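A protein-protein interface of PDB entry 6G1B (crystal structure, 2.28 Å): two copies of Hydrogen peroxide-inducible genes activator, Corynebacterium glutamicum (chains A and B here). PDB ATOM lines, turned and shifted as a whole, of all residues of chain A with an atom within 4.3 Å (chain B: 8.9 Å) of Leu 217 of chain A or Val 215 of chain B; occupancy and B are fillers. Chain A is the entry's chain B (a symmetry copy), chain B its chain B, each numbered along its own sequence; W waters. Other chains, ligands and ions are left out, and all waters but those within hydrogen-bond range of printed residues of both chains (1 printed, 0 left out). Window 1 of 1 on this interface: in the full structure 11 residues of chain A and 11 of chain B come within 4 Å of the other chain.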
ATOM      1  N   LEU A 193     -23.622  -2.912  -6.973  1.00  0.00           N
ATOM      2  CA  LEU A 193     -22.334  -3.138  -7.638  1.00  0.00           C
ATOM      3  C   LEU A 193     -21.130  -2.881  -6.731  1.00  0.00           C
ATOM      4  O   LEU A 193     -20.134  -3.606  -6.811  1.00  0.00           O
ATOM      5  CB  LEU A 193     -22.192  -2.348  -8.932  1.00  0.00           C
ATOM      6  CG  LEU A 193     -22.836  -2.948 -10.176  1.00  0.00           C
ATOM      7  CD1 LEU A 193     -22.469  -2.183 -11.431  1.00  0.00           C
ATOM      8  CD2 LEU A 193     -22.525  -4.425 -10.359  1.00  0.00           C
ATOM      9  N   LEU A 196     -18.867  -5.706  -5.106  1.00  0.00           N
ATOM     10  CA  LEU A 196     -17.691  -6.288  -5.796  1.00  0.00           C
ATOM     11  C   LEU A 196     -16.396  -6.125  -5.010  1.00  0.00           C
ATOM     12  O   LEU A 196     -15.583  -7.056  -4.947  1.00  0.00           O
ATOM     13  CB  LEU A 196     -17.468  -5.614  -7.147  1.00  0.00           C
ATOM     14  CG  LEU A 196     -18.500  -5.861  -8.229  1.00  0.00           C
ATOM     15  CD1 LEU A 196     -18.191  -5.008  -9.437  1.00  0.00           C
ATOM     16  CD2 LEU A 196     -18.488  -7.302  -8.623  1.00  0.00           C
ATOM     17  N   GLU A 197     -16.252  -4.971  -4.367  1.00  0.00           N
ATOM     18  CA  GLU A 197     -15.060  -4.636  -3.608  1.00  0.00           C
ATOM     19  C   GLU A 197     -14.814  -5.551  -2.410  1.00  0.00           C
ATOM     20  O   GLU A 197     -13.676  -5.595  -1.920  1.00  0.00           O
ATOM     21  CB  GLU A 197     -15.147  -3.201  -3.068  1.00  0.00           C
ATOM     22  CG  GLU A 197     -15.440  -2.136  -4.114  1.00  0.00           C
ATOM     23  CD  GLU A 197     -14.246  -1.700  -4.917  1.00  0.00           C
ATOM     24  OE1 GLU A 197     -14.474  -1.321  -6.098  1.00  0.00           O
ATOM     25  OE2 GLU A 197     -13.109  -1.684  -4.364  1.00  0.00           O
ATOM     26  N   LEU A 210     -22.355  -7.212 -16.186  1.00  0.00           N
ATOM     27  CA  LEU A 210     -22.685  -6.538 -14.919  1.00  0.00           C
ATOM     28  C   LEU A 210     -22.765  -5.033 -15.119  1.00  0.00           C
ATOM     29  O   LEU A 210     -21.802  -4.416 -15.581  1.00  0.00           O
ATOM     30  CB  LEU A 210     -21.658  -6.864 -13.814  1.00  0.00           C
ATOM     31  CG  LEU A 210     -22.149  -7.779 -12.675  1.00  0.00           C
ATOM     32  CD1 LEU A 210     -22.480  -9.161 -13.192  1.00  0.00           C
ATOM     33  CD2 LEU A 210     -21.111  -7.896 -11.576  1.00  0.00           C
ATOM     34  N   VAL A 215     -23.079   2.873 -13.501  1.00  0.00           N
ATOM     35  CA  VAL A 215     -21.784   2.229 -13.788  1.00  0.00           C
ATOM     36  C   VAL A 215     -21.976   1.032 -14.744  1.00  0.00           C
ATOM     37  O   VAL A 215     -22.851   0.216 -14.536  1.00  0.00           O
ATOM     38  CB  VAL A 215     -21.114   1.779 -12.464  1.00  0.00           C
ATOM     39  CG1 VAL A 215     -20.027   0.744 -12.676  1.00  0.00           C
ATOM     40  CG2 VAL A 215     -20.550   2.971 -11.705  1.00  0.00           C
ATOM     41  N   ASP A 216     -21.159   0.960 -15.789  1.00  0.00           N
ATOM     42  CA  ASP A 216     -21.169  -0.144 -16.750  1.00  0.00           C
ATOM     43  C   ASP A 216     -19.833  -0.898 -16.702  1.00  0.00           C
ATOM     44  O   ASP A 216     -18.817  -0.345 -17.090  1.00  0.00           O
ATOM     45  CB  ASP A 216     -21.468   0.358 -18.175  1.00  0.00           C
ATOM     46  CG  ASP A 216     -21.775  -0.787 -19.147  1.00  0.00           C
ATOM     47  OD1 ASP A 216     -21.033  -1.766 -19.128  1.00  0.00           O
ATOM     48  OD2 ASP A 216     -22.739  -0.722 -19.918  1.00  0.00           O
ATOM     49  N   LEU A 217     -19.852  -2.134 -16.187  1.00  0.00           N
ATOM     50  CA  LEU A 217     -18.663  -2.984 -16.095  1.00  0.00           C
ATOM     51  C   LEU A 217     -18.685  -4.090 -17.152  1.00  0.00           C
ATOM     52  O   LEU A 217     -17.815  -4.960 -17.183  1.00  0.00           O
ATOM     53  CB  LEU A 217     -18.549  -3.593 -14.694  1.00  0.00           C
ATOM     54  CG  LEU A 217     -18.573  -2.595 -13.535  1.00  0.00           C
ATOM     55  CD1 LEU A 217     -18.536  -3.284 -12.203  1.00  0.00           C
ATOM     56  CD2 LEU A 217     -17.415  -1.612 -13.662  1.00  0.00           C
ATOM     57  N   CYS A 218     -19.692  -4.047 -18.012  1.00  0.00           N
ATOM     58  CA  CYS A 218     -19.862  -5.010 -19.063  1.00  0.00           C
ATOM     59  C   CYS A 218     -18.961  -4.633 -20.244  1.00  0.00           C
ATOM     60  O   CYS A 218     -17.878  -5.229 -20.387  1.00  0.00           O
ATOM     61  CB  CYS A 218     -21.343  -5.053 -19.427  1.00  0.00           C
ATOM     62  SG  CYS A 218     -21.816  -6.405 -20.501  1.00  0.00           S
ATOM     63  N   ARG A 219     -19.351  -3.584 -20.988  1.00  0.00           N
ATOM     64  CA  ARG A 219     -18.879  -3.293 -22.365  1.00  0.00           C
ATOM     65  C   ARG A 219     -17.423  -3.678 -22.593  1.00  0.00           C
ATOM     66  O   ARG A 219     -16.535  -2.835 -22.503  1.00  0.00           O
ATOM     67  CB  ARG A 219     -19.052  -1.799 -22.746  1.00  0.00           C
ATOM     68  CG  ARG A 219     -20.448  -1.161 -22.715  1.00  0.00           C
ATOM     69  CD  ARG A 219     -21.667  -2.085 -22.637  1.00  0.00           C
ATOM     70  NE  ARG A 219     -21.703  -3.188 -23.603  1.00  0.00           N
ATOM     71  CZ  ARG A 219     -21.983  -3.082 -24.907  1.00  0.00           C
ATOM     72  NH1 ARG A 219     -22.256  -1.902 -25.475  1.00  0.00           N
ATOM     73  NH2 ARG A 219     -21.984  -4.184 -25.662  1.00  0.00           N
ATOM     74  N   PRO A 225     -12.626  -4.697 -17.055  1.00  0.00           N
ATOM     75  CA  PRO A 225     -12.577  -3.617 -16.041  1.00  0.00           C
ATOM     76  C   PRO A 225     -12.629  -4.119 -14.588  1.00  0.00           C
ATOM     77  O   PRO A 225     -12.171  -3.394 -13.680  1.00  0.00           O
ATOM     78  CB  PRO A 225     -13.791  -2.748 -16.381  1.00  0.00           C
ATOM     79  CG  PRO A 225     -14.751  -3.691 -16.987  1.00  0.00           C
ATOM     80  CD  PRO A 225     -13.951  -4.775 -17.686  1.00  0.00           C
ATOM     81  N   ILE A 226     -13.155  -5.330 -14.372  1.00  0.00           N
ATOM     82  CA  ILE A 226     -13.073  -5.963 -13.059  1.00  0.00           C
ATOM     83  C   ILE A 226     -11.766  -6.739 -12.981  1.00  0.00           C
ATOM     84  O   ILE A 226     -11.482  -7.560 -13.829  1.00  0.00           O
ATOM     85  CB  ILE A 226     -14.263  -6.903 -12.780  1.00  0.00           C
ATOM     86  CG1 ILE A 226     -15.589  -6.137 -12.861  1.00  0.00           C
ATOM     87  CG2 ILE A 226     -14.125  -7.535 -11.402  1.00  0.00           C
ATOM     88  CD1 ILE A 226     -16.814  -7.017 -12.997  1.00  0.00           C
ATOM     89  N   LEU B 193     -15.363   4.064  -4.546  1.00  0.00           N
ATOM     90  CA  LEU B 193     -15.988   4.196  -5.867  1.00  0.00           C
ATOM     91  C   LEU B 193     -17.502   3.984  -5.845  1.00  0.00           C
ATOM     92  O   LEU B 193     -18.231   4.670  -6.567  1.00  0.00           O
ATOM     93  CB  LEU B 193     -15.348   3.296  -6.915  1.00  0.00           C
ATOM     94  CG  LEU B 193     -14.070   3.806  -7.570  1.00  0.00           C
ATOM     95  CD1 LEU B 193     -13.634   2.926  -8.724  1.00  0.00           C
ATOM     96  CD2 LEU B 193     -14.167   5.252  -8.027  1.00  0.00           C
ATOM     97  N   SER B 194     -17.984   3.096  -4.992  1.00  0.00           N
ATOM     98  CA  SER B 194     -19.433   2.963  -4.769  1.00  0.00           C
ATOM     99  C   SER B 194     -20.201   4.278  -4.500  1.00  0.00           C
ATOM    100  O   SER B 194     -21.404   4.348  -4.755  1.00  0.00           O
ATOM    101  CB  SER B 194     -19.712   2.027  -3.597  1.00  0.00           C
ATOM    102  OG  SER B 194     -19.251   2.572  -2.382  1.00  0.00           O
ATOM    103  N   LEU B 196     -20.207   6.871  -6.147  1.00  0.00           N
ATOM    104  CA  LEU B 196     -20.717   7.358  -7.451  1.00  0.00           C
ATOM    105  C   LEU B 196     -22.228   7.226  -7.588  1.00  0.00           C
ATOM    106  O   LEU B 196     -22.891   8.135  -8.104  1.00  0.00           O
ATOM    107  CB  LEU B 196     -20.105   6.566  -8.603  1.00  0.00           C
ATOM    108  CG  LEU B 196     -18.624   6.749  -8.867  1.00  0.00           C
ATOM    109  CD1 LEU B 196     -18.171   5.788  -9.941  1.00  0.00           C
ATOM    110  CD2 LEU B 196     -18.356   8.151  -9.309  1.00  0.00           C
ATOM    111  N   GLU B 197     -22.762   6.128  -7.065  1.00  0.00           N
ATOM    112  CA  GLU B 197     -24.180   5.824  -7.146  1.00  0.00           C
ATOM    113  C   GLU B 197     -25.069   6.831  -6.419  1.00  0.00           C
ATOM    114  O   GLU B 197     -26.272   6.883  -6.714  1.00  0.00           O
ATOM    115  CB  GLU B 197     -24.475   4.444  -6.542  1.00  0.00           C
ATOM    116  CG  GLU B 197     -23.644   3.302  -7.109  1.00  0.00           C
ATOM    117  CD  GLU B 197     -24.129   2.765  -8.427  1.00  0.00           C
ATOM    118  OE1 GLU B 197     -23.250   2.295  -9.198  1.00  0.00           O
ATOM    119  OE2 GLU B 197     -25.372   2.765  -8.667  1.00  0.00           O
ATOM    120  N   CYS B 209      -9.597  10.287 -14.422  1.00  0.00           N
ATOM    121  CA  CYS B 209      -9.287   8.861 -14.466  1.00  0.00           C
ATOM    122  C   CYS B 209      -9.621   8.271 -13.079  1.00  0.00           C
ATOM    123  O   CYS B 209      -8.895   8.521 -12.105  1.00  0.00           O
ATOM    124  CB  CYS B 209      -7.804   8.701 -14.803  1.00  0.00           C
ATOM    125  SG  CYS B 209      -7.176   6.999 -14.832  1.00  0.00           S
ATOM    126  N   LEU B 210     -10.732   7.529 -13.003  1.00  0.00           N
ATOM    127  CA  LEU B 210     -11.247   6.974 -11.740  1.00  0.00           C
ATOM    128  C   LEU B 210     -11.105   5.461 -11.724  1.00  0.00           C
ATOM    129  O   LEU B 210     -11.616   4.779 -12.616  1.00  0.00           O
ATOM    130  CB  LEU B 210     -12.721   7.363 -11.504  1.00  0.00           C
ATOM    131  CG  LEU B 210     -12.985   8.385 -10.381  1.00  0.00           C
ATOM    132  CD1 LEU B 210     -12.371   9.727 -10.711  1.00  0.00           C
ATOM    133  CD2 LEU B 210     -14.471   8.566 -10.138  1.00  0.00           C
ATOM    134  N   HIS B 211     -10.410   4.940 -10.719  1.00  0.00           N
ATOM    135  CA  HIS B 211     -10.294   3.477 -10.515  1.00  0.00           C
ATOM    136  C   HIS B 211      -9.796   3.196  -9.099  1.00  0.00           C
ATOM    137  O   HIS B 211      -9.198   4.077  -8.436  1.00  0.00           O
ATOM    138  CB  HIS B 211      -9.353   2.804 -11.563  1.00  0.00           C
ATOM    139  CG  HIS B 211      -7.938   3.282 -11.507  1.00  0.00           C
ATOM    140  ND1 HIS B 211      -7.448   4.290 -12.309  1.00  0.00           N
ATOM    141  CD2 HIS B 211      -6.912   2.917 -10.704  1.00  0.00           C
ATOM    142  CE1 HIS B 211      -6.180   4.516 -12.012  1.00  0.00           C
ATOM    143  NE2 HIS B 211      -5.837   3.704 -11.033  1.00  0.00           N
ATOM    144  N   ASP B 212     -10.035   1.961  -8.658  1.00  0.00           N
ATOM    145  CA  ASP B 212      -9.380   1.368  -7.479  1.00  0.00           C
ATOM    146  C   ASP B 212      -8.813   0.018  -7.913  1.00  0.00           C
ATOM    147  O   ASP B 212      -8.834  -0.281  -9.104  1.00  0.00           O
ATOM    148  CB  ASP B 212     -10.354   1.272  -6.289  1.00  0.00           C
ATOM    149  CG  ASP B 212     -11.566   0.343  -6.562  1.00  0.00           C
ATOM    150  OD1 ASP B 212     -11.453  -0.602  -7.368  1.00  0.00           O
ATOM    151  OD2 ASP B 212     -12.642   0.573  -5.970  1.00  0.00           O
ATOM    152  N   GLN B 213      -8.351  -0.809  -6.976  1.00  0.00           N
ATOM    153  CA  GLN B 213      -7.636  -2.071  -7.323  1.00  0.00           C
ATOM    154  C   GLN B 213      -8.500  -3.144  -7.985  1.00  0.00           C
ATOM    155  O   GLN B 213      -7.969  -4.087  -8.583  1.00  0.00           O
ATOM    156  CB  GLN B 213      -6.953  -2.676  -6.084  1.00  0.00           C
ATOM    157  CG  GLN B 213      -5.848  -1.809  -5.466  1.00  0.00           C
ATOM    158  CD  GLN B 213      -6.348  -0.908  -4.333  1.00  0.00           C
ATOM    159  OE1 GLN B 213      -6.976   0.133  -4.592  1.00  0.00           O
ATOM    160  NE2 GLN B 213      -6.094  -1.312  -3.072  1.00  0.00           N
ATOM    161  N   ILE B 214      -9.822  -3.013  -7.864  1.00  0.00           N
ATOM    162  CA  ILE B 214     -10.789  -4.007  -8.366  1.00  0.00           C
ATOM    163  C   ILE B 214     -11.591  -3.526  -9.588  1.00  0.00           C
ATOM    164  O   ILE B 214     -11.786  -4.296 -10.507  1.00  0.00           O
ATOM    165  CB  ILE B 214     -11.738  -4.404  -7.215  1.00  0.00           C
ATOM    166  CG1 ILE B 214     -10.921  -5.010  -6.059  1.00  0.00           C
ATOM    167  CG2 ILE B 214     -12.786  -5.406  -7.688  1.00  0.00           C
ATOM    168  CD1 ILE B 214     -11.592  -4.953  -4.714  1.00  0.00           C
ATOM    169  N   VAL B 215     -12.049  -2.268  -9.576  1.00  0.00           N
ATOM    170  CA  VAL B 215     -12.894  -1.687 -10.635  1.00  0.00           C
ATOM    171  C   VAL B 215     -12.133  -0.571 -11.383  1.00  0.00           C
ATOM    172  O   VAL B 215     -11.535   0.285 -10.762  1.00  0.00           O
ATOM    173  CB  VAL B 215     -14.210  -1.146 -10.022  1.00  0.00           C
ATOM    174  CG1 VAL B 215     -14.924  -0.163 -10.930  1.00  0.00           C
ATOM    175  CG2 VAL B 215     -15.150  -2.285  -9.655  1.00  0.00           C
ATOM    176  N   ASP B 216     -12.158  -0.611 -12.711  1.00  0.00           N
ATOM    177  CA  ASP B 216     -11.543   0.408 -13.563  1.00  0.00           C
ATOM    178  C   ASP B 216     -12.619   1.125 -14.390  1.00  0.00           C
ATOM    179  O   ASP B 216     -13.215   0.512 -15.261  1.00  0.00           O
ATOM    180  CB  ASP B 216     -10.464  -0.205 -14.475  1.00  0.00           C
ATOM    181  CG  ASP B 216      -9.603   0.861 -15.163  1.00  0.00           C
ATOM    182  OD1 ASP B 216     -10.180   1.817 -15.675  1.00  0.00           O
ATOM    183  OD2 ASP B 216      -8.372   0.759 -15.192  1.00  0.00           O
ATOM    184  N   LEU B 217     -12.877   2.400 -14.073  1.00  0.00           N
ATOM    185  CA  LEU B 217     -13.860   3.221 -14.785  1.00  0.00           C
ATOM    186  C   LEU B 217     -13.177   4.233 -15.707  1.00  0.00           C
ATOM    187  O   LEU B 217     -13.830   5.073 -16.327  1.00  0.00           O
ATOM    188  CB  LEU B 217     -14.773   3.943 -13.790  1.00  0.00           C
ATOM    189  CG  LEU B 217     -15.477   3.048 -12.768  1.00  0.00           C
ATOM    190  CD1 LEU B 217     -16.285   3.847 -11.789  1.00  0.00           C
ATOM    191  CD2 LEU B 217     -16.355   2.025 -13.480  1.00  0.00           C
ATOM    192  N   CYS B 218     -11.858   4.146 -15.785  1.00  0.00           N
ATOM    193  CA  CYS B 218     -11.065   5.020 -16.601  1.00  0.00           C
ATOM    194  C   CYS B 218     -11.087   4.519 -18.049  1.00  0.00           C
ATOM    195  O   CYS B 218     -11.851   5.069 -18.862  1.00  0.00           O
ATOM    196  CB  CYS B 218      -9.660   5.075 -16.007  1.00  0.00           C
ATOM    197  SG  CYS B 218      -8.600   6.343 -16.692  1.00  0.00           S
ATOM    198  N   ARG B 219     -10.360   3.422 -18.318  1.00  0.00           N
ATOM    199  CA  ARG B 219      -9.919   3.002 -19.672  1.00  0.00           C
ATOM    200  C   ARG B 219     -10.937   3.325 -20.759  1.00  0.00           C
ATOM    201  O   ARG B 219     -11.725   2.468 -21.149  1.00  0.00           O
ATOM    202  CB  ARG B 219      -9.595   1.486 -19.745  1.00  0.00           C
ATOM    203  CG  ARG B 219      -8.515   0.893 -18.829  1.00  0.00           C
ATOM    204  CD  ARG B 219      -7.560   1.855 -18.115  1.00  0.00           C
ATOM    205  NE  ARG B 219      -6.922   2.872 -18.957  1.00  0.00           N
ATOM    206  CZ  ARG B 219      -5.919   2.663 -19.817  1.00  0.00           C
ATOM    207  NH1 ARG B 219      -5.393   1.448 -20.005  1.00  0.00           N
ATOM    208  NH2 ARG B 219      -5.435   3.698 -20.511  1.00  0.00           N
ATOM    209  N   ASN B 224     -18.199   5.759 -22.525  1.00  0.00           N
ATOM    210  CA  ASN B 224     -18.042   6.280 -21.172  1.00  0.00           C
ATOM    211  C   ASN B 224     -18.781   5.336 -20.242  1.00  0.00           C
ATOM    212  O   ASN B 224     -19.983   5.190 -20.379  1.00  0.00           O
ATOM    213  CB  ASN B 224     -18.603   7.708 -21.095  1.00  0.00           C
ATOM    214  CG  ASN B 224     -18.502   8.322 -19.704  1.00  0.00           C
ATOM    215  OD1 ASN B 224     -17.934   7.741 -18.776  1.00  0.00           O
ATOM    216  ND2 ASN B 224     -19.076   9.507 -19.552  1.00  0.00           N
ATOM    217  N   PRO B 225     -18.065   4.674 -19.314  1.00  0.00           N
ATOM    218  CA  PRO B 225     -18.743   3.684 -18.444  1.00  0.00           C
ATOM    219  C   PRO B 225     -19.558   4.308 -17.300  1.00  0.00           C
ATOM    220  O   PRO B 225     -20.489   3.650 -16.789  1.00  0.00           O
ATOM    221  CB  PRO B 225     -17.592   2.823 -17.913  1.00  0.00           C
ATOM    222  CG  PRO B 225     -16.435   3.738 -17.900  1.00  0.00           C
ATOM    223  CD  PRO B 225     -16.625   4.736 -19.028  1.00  0.00           C
ATOM    224  N   ILE B 226     -19.232   5.548 -16.915  1.00  0.00           N
ATOM    225  CA  ILE B 226     -20.066   6.287 -15.973  1.00  0.00           C
ATOM    226  C   ILE B 226     -21.137   7.030 -16.760  1.00  0.00           C
ATOM    227  O   ILE B 226     -20.833   7.767 -17.674  1.00  0.00           O
ATOM    228  CB  ILE B 226     -19.256   7.280 -15.117  1.00  0.00           C
ATOM    229  CG1 ILE B 226     -18.168   6.549 -14.321  1.00  0.00           C
ATOM    230  CG2 ILE B 226     -20.174   8.023 -14.156  1.00  0.00           C
ATOM    231  CD1 ILE B 226     -17.082   7.448 -13.770  1.00  0.00           C
ATOM    232  N   ASP B 276      -7.050   4.507  -1.366  1.00  0.00           N
ATOM    233  CA  ASP B 276      -6.987   3.414  -2.335  1.00  0.00           C
ATOM    234  C   ASP B 276      -7.643   3.741  -3.677  1.00  0.00           C
ATOM    235  O   ASP B 276      -7.459   3.004  -4.646  1.00  0.00           O
ATOM    236  CB  ASP B 276      -7.521   2.083  -1.760  1.00  0.00           C
ATOM    237  CG  ASP B 276      -8.803   2.226  -0.934  1.00  0.00           C
ATOM    238  OD1 ASP B 276      -9.621   3.164  -1.213  1.00  0.00           O
ATOM    239  OD2 ASP B 276      -8.979   1.390   0.016  1.00  0.00           O
ATOM    240  N   VAL B 277      -8.418   4.813  -3.745  1.00  0.00           N
ATOM    241  CA  VAL B 277      -9.019   5.235  -5.004  1.00  0.00           C
ATOM    242  C   VAL B 277      -8.062   6.163  -5.725  1.00  0.00           C
ATOM    243  O   VAL B 277      -7.459   7.034  -5.122  1.00  0.00           O
ATOM    244  CB  VAL B 277     -10.372   5.923  -4.767  1.00  0.00           C
ATOM    245  CG1 VAL B 277     -10.972   6.432  -6.060  1.00  0.00           C
ATOM    246  CG2 VAL B 277     -11.335   4.940  -4.104  1.00  0.00           C
ATOM    247  N   THR B 278      -7.903   5.946  -7.018  1.00  0.00           N
ATOM    248  CA  THR B 278      -7.249   6.921  -7.888  1.00  0.00           C
ATOM    249  C   THR B 278      -8.345   7.788  -8.499  1.00  0.00           C
ATOM    250  O   THR B 278      -9.305   7.264  -9.074  1.00  0.00           O
ATOM    251  CB  THR B 278      -6.405   6.240  -8.977  1.00  0.00           C
ATOM    252  OG1 THR B 278      -5.277   5.625  -8.356  1.00  0.00           O
ATOM    253  CG2 THR B 278      -5.879   7.279 -10.021  1.00  0.00           C
HETATM  254  O   HOH W   1      -9.762  -3.222 -12.543  1.00  0.00           O
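The backbone NH (N) of Asp 216 of chain B is in hydrogen-bond range of the backbone carbonyl oxygen (O) of Pro 225 of chain A (2.9 Å).
O of Ile 214 of chain B lies close to O of Pro 225 of chain A (3.3 Å).
The backbone carbonyl oxygen of Pro 225 of chain B sits at hydrogen-bond distance from the backbone NH of Asp 216 of chain A (2.9 Å).
OE1 of Glu 197 of chain A sits close to OD2 of Asp 212 of chain B (2.6 Å).
N of Leu 217 of chain B is in hydrogen-bond range of O of Leu 210 of chain B (3.1 Å).
OD1 of Asp 212 of chain B is in hydrogen-bond range of N of Val 215 of chain B (2.8 Å).
The side-chain carboxylate (OD1) of Asp 216 of chain B is in hydrogen-bond range of the backbone NH (N) of Cys 218 of chain B (2.9 Å).
SG of Cys 218 of chain B is disulfide-bonded to SG of Cys 209 of chain B (2.4 Å).
The side-chain carboxylate (OD1) of Asp 216 of chain A sits at hydrogen-bond distance from the backbone NH (N) of Arg 219 of chain A (3.1 Å).
N of Ile 214 of chain B sits at hydrogen-bond distance from OD1 of Asp 212 of chain B (3.0 Å).
Among the printed residues, merely in contact across the chains: Ile 226 of chain A with Ile 214 of chain B (3.3 Å), Glu 197 of chain A with Ile 214 of chain B (3.5 Å), Val 215 of chain A with Pro 225 of chain B (3.6 Å), Pro 225 of chain A with Val 215 of chain B (3.6 Å), Val 215 of chain A with Glu 197 of chain B (3.7 Å), Glu 197 of chain A with Val 215 of chain B (3.7 Å), Leu 217 of chain A with Leu 217 of chain B (3.8 Å), Leu 217 of chain A with Val 215 of chain B (3.97 Å) and Val 215 of chain A with Leu 217 of chain B (3.97 Å).
Leu 217 of chain A touches just these residues of chain B: Val 215 (3.97 Å) and Leu 217 (3.8 Å).
Val 215 of chain B touches just these residues of chain A: Glu 197, Leu 217 and Pro 225.
Of the printed residues of chain A, Glu 197 of chain B touches Val 215.
Of the printed residues of chain A, Asp 212 of chain B touches Glu 197.
Asp 276 of chain B touches none of the printed residues of chain A.
Leu 196 of chain A touches none of the printed residues of chain B.
The nearest residue of chain B that does not touch Leu 217 of chain A is Asp 216 of chain B (5.0 Å).
Printed residues of chain A that touch a printed residue of chain B: Glu 197, Val 215, Asp 216, Leu 217, Pro 225 and Ile 226.
Printed residues of chain B that touch a printed residue of chain A: Glu 197, Asp 212, Ile 214, Val 215, Asp 216, Leu 217 and Pro 225.
Hydrophobic or aromatic side chains of chain B within 4 Å of the printed part of chain A: Ile 214, Val 215, Leu 217 and Pro 225.
Along chain B the printed residues that touch a printed residue of chain A span positions 197 to 225.
Among the printed residues, 13 pairs touch across the chains.
Glu 197 of chain A touches Val 215 of chain B, and with the chains exchanged Val 215 of chain A touches Glu 197 of chain B.
Val 215 of chain A touches Leu 217 of chain B, and with the chains exchanged Leu 217 of chain A touches Val 215 of chain B.
Val 215 of chain A touches Pro 225 of chain B, and with the chains exchanged Pro 225 of chain A touches Val 215 of chain B.
Leu 217 of chain A touches its own counterpart, Leu 217 of chain B.
Water W1 lies within hydrogen-bond range of the backbone carbonyl oxygen (O) of Pro 225 of chain A (2.7 Å) and the backbone carbonyl oxygen (O) of Ile 214 of chain B (3.1 Å).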
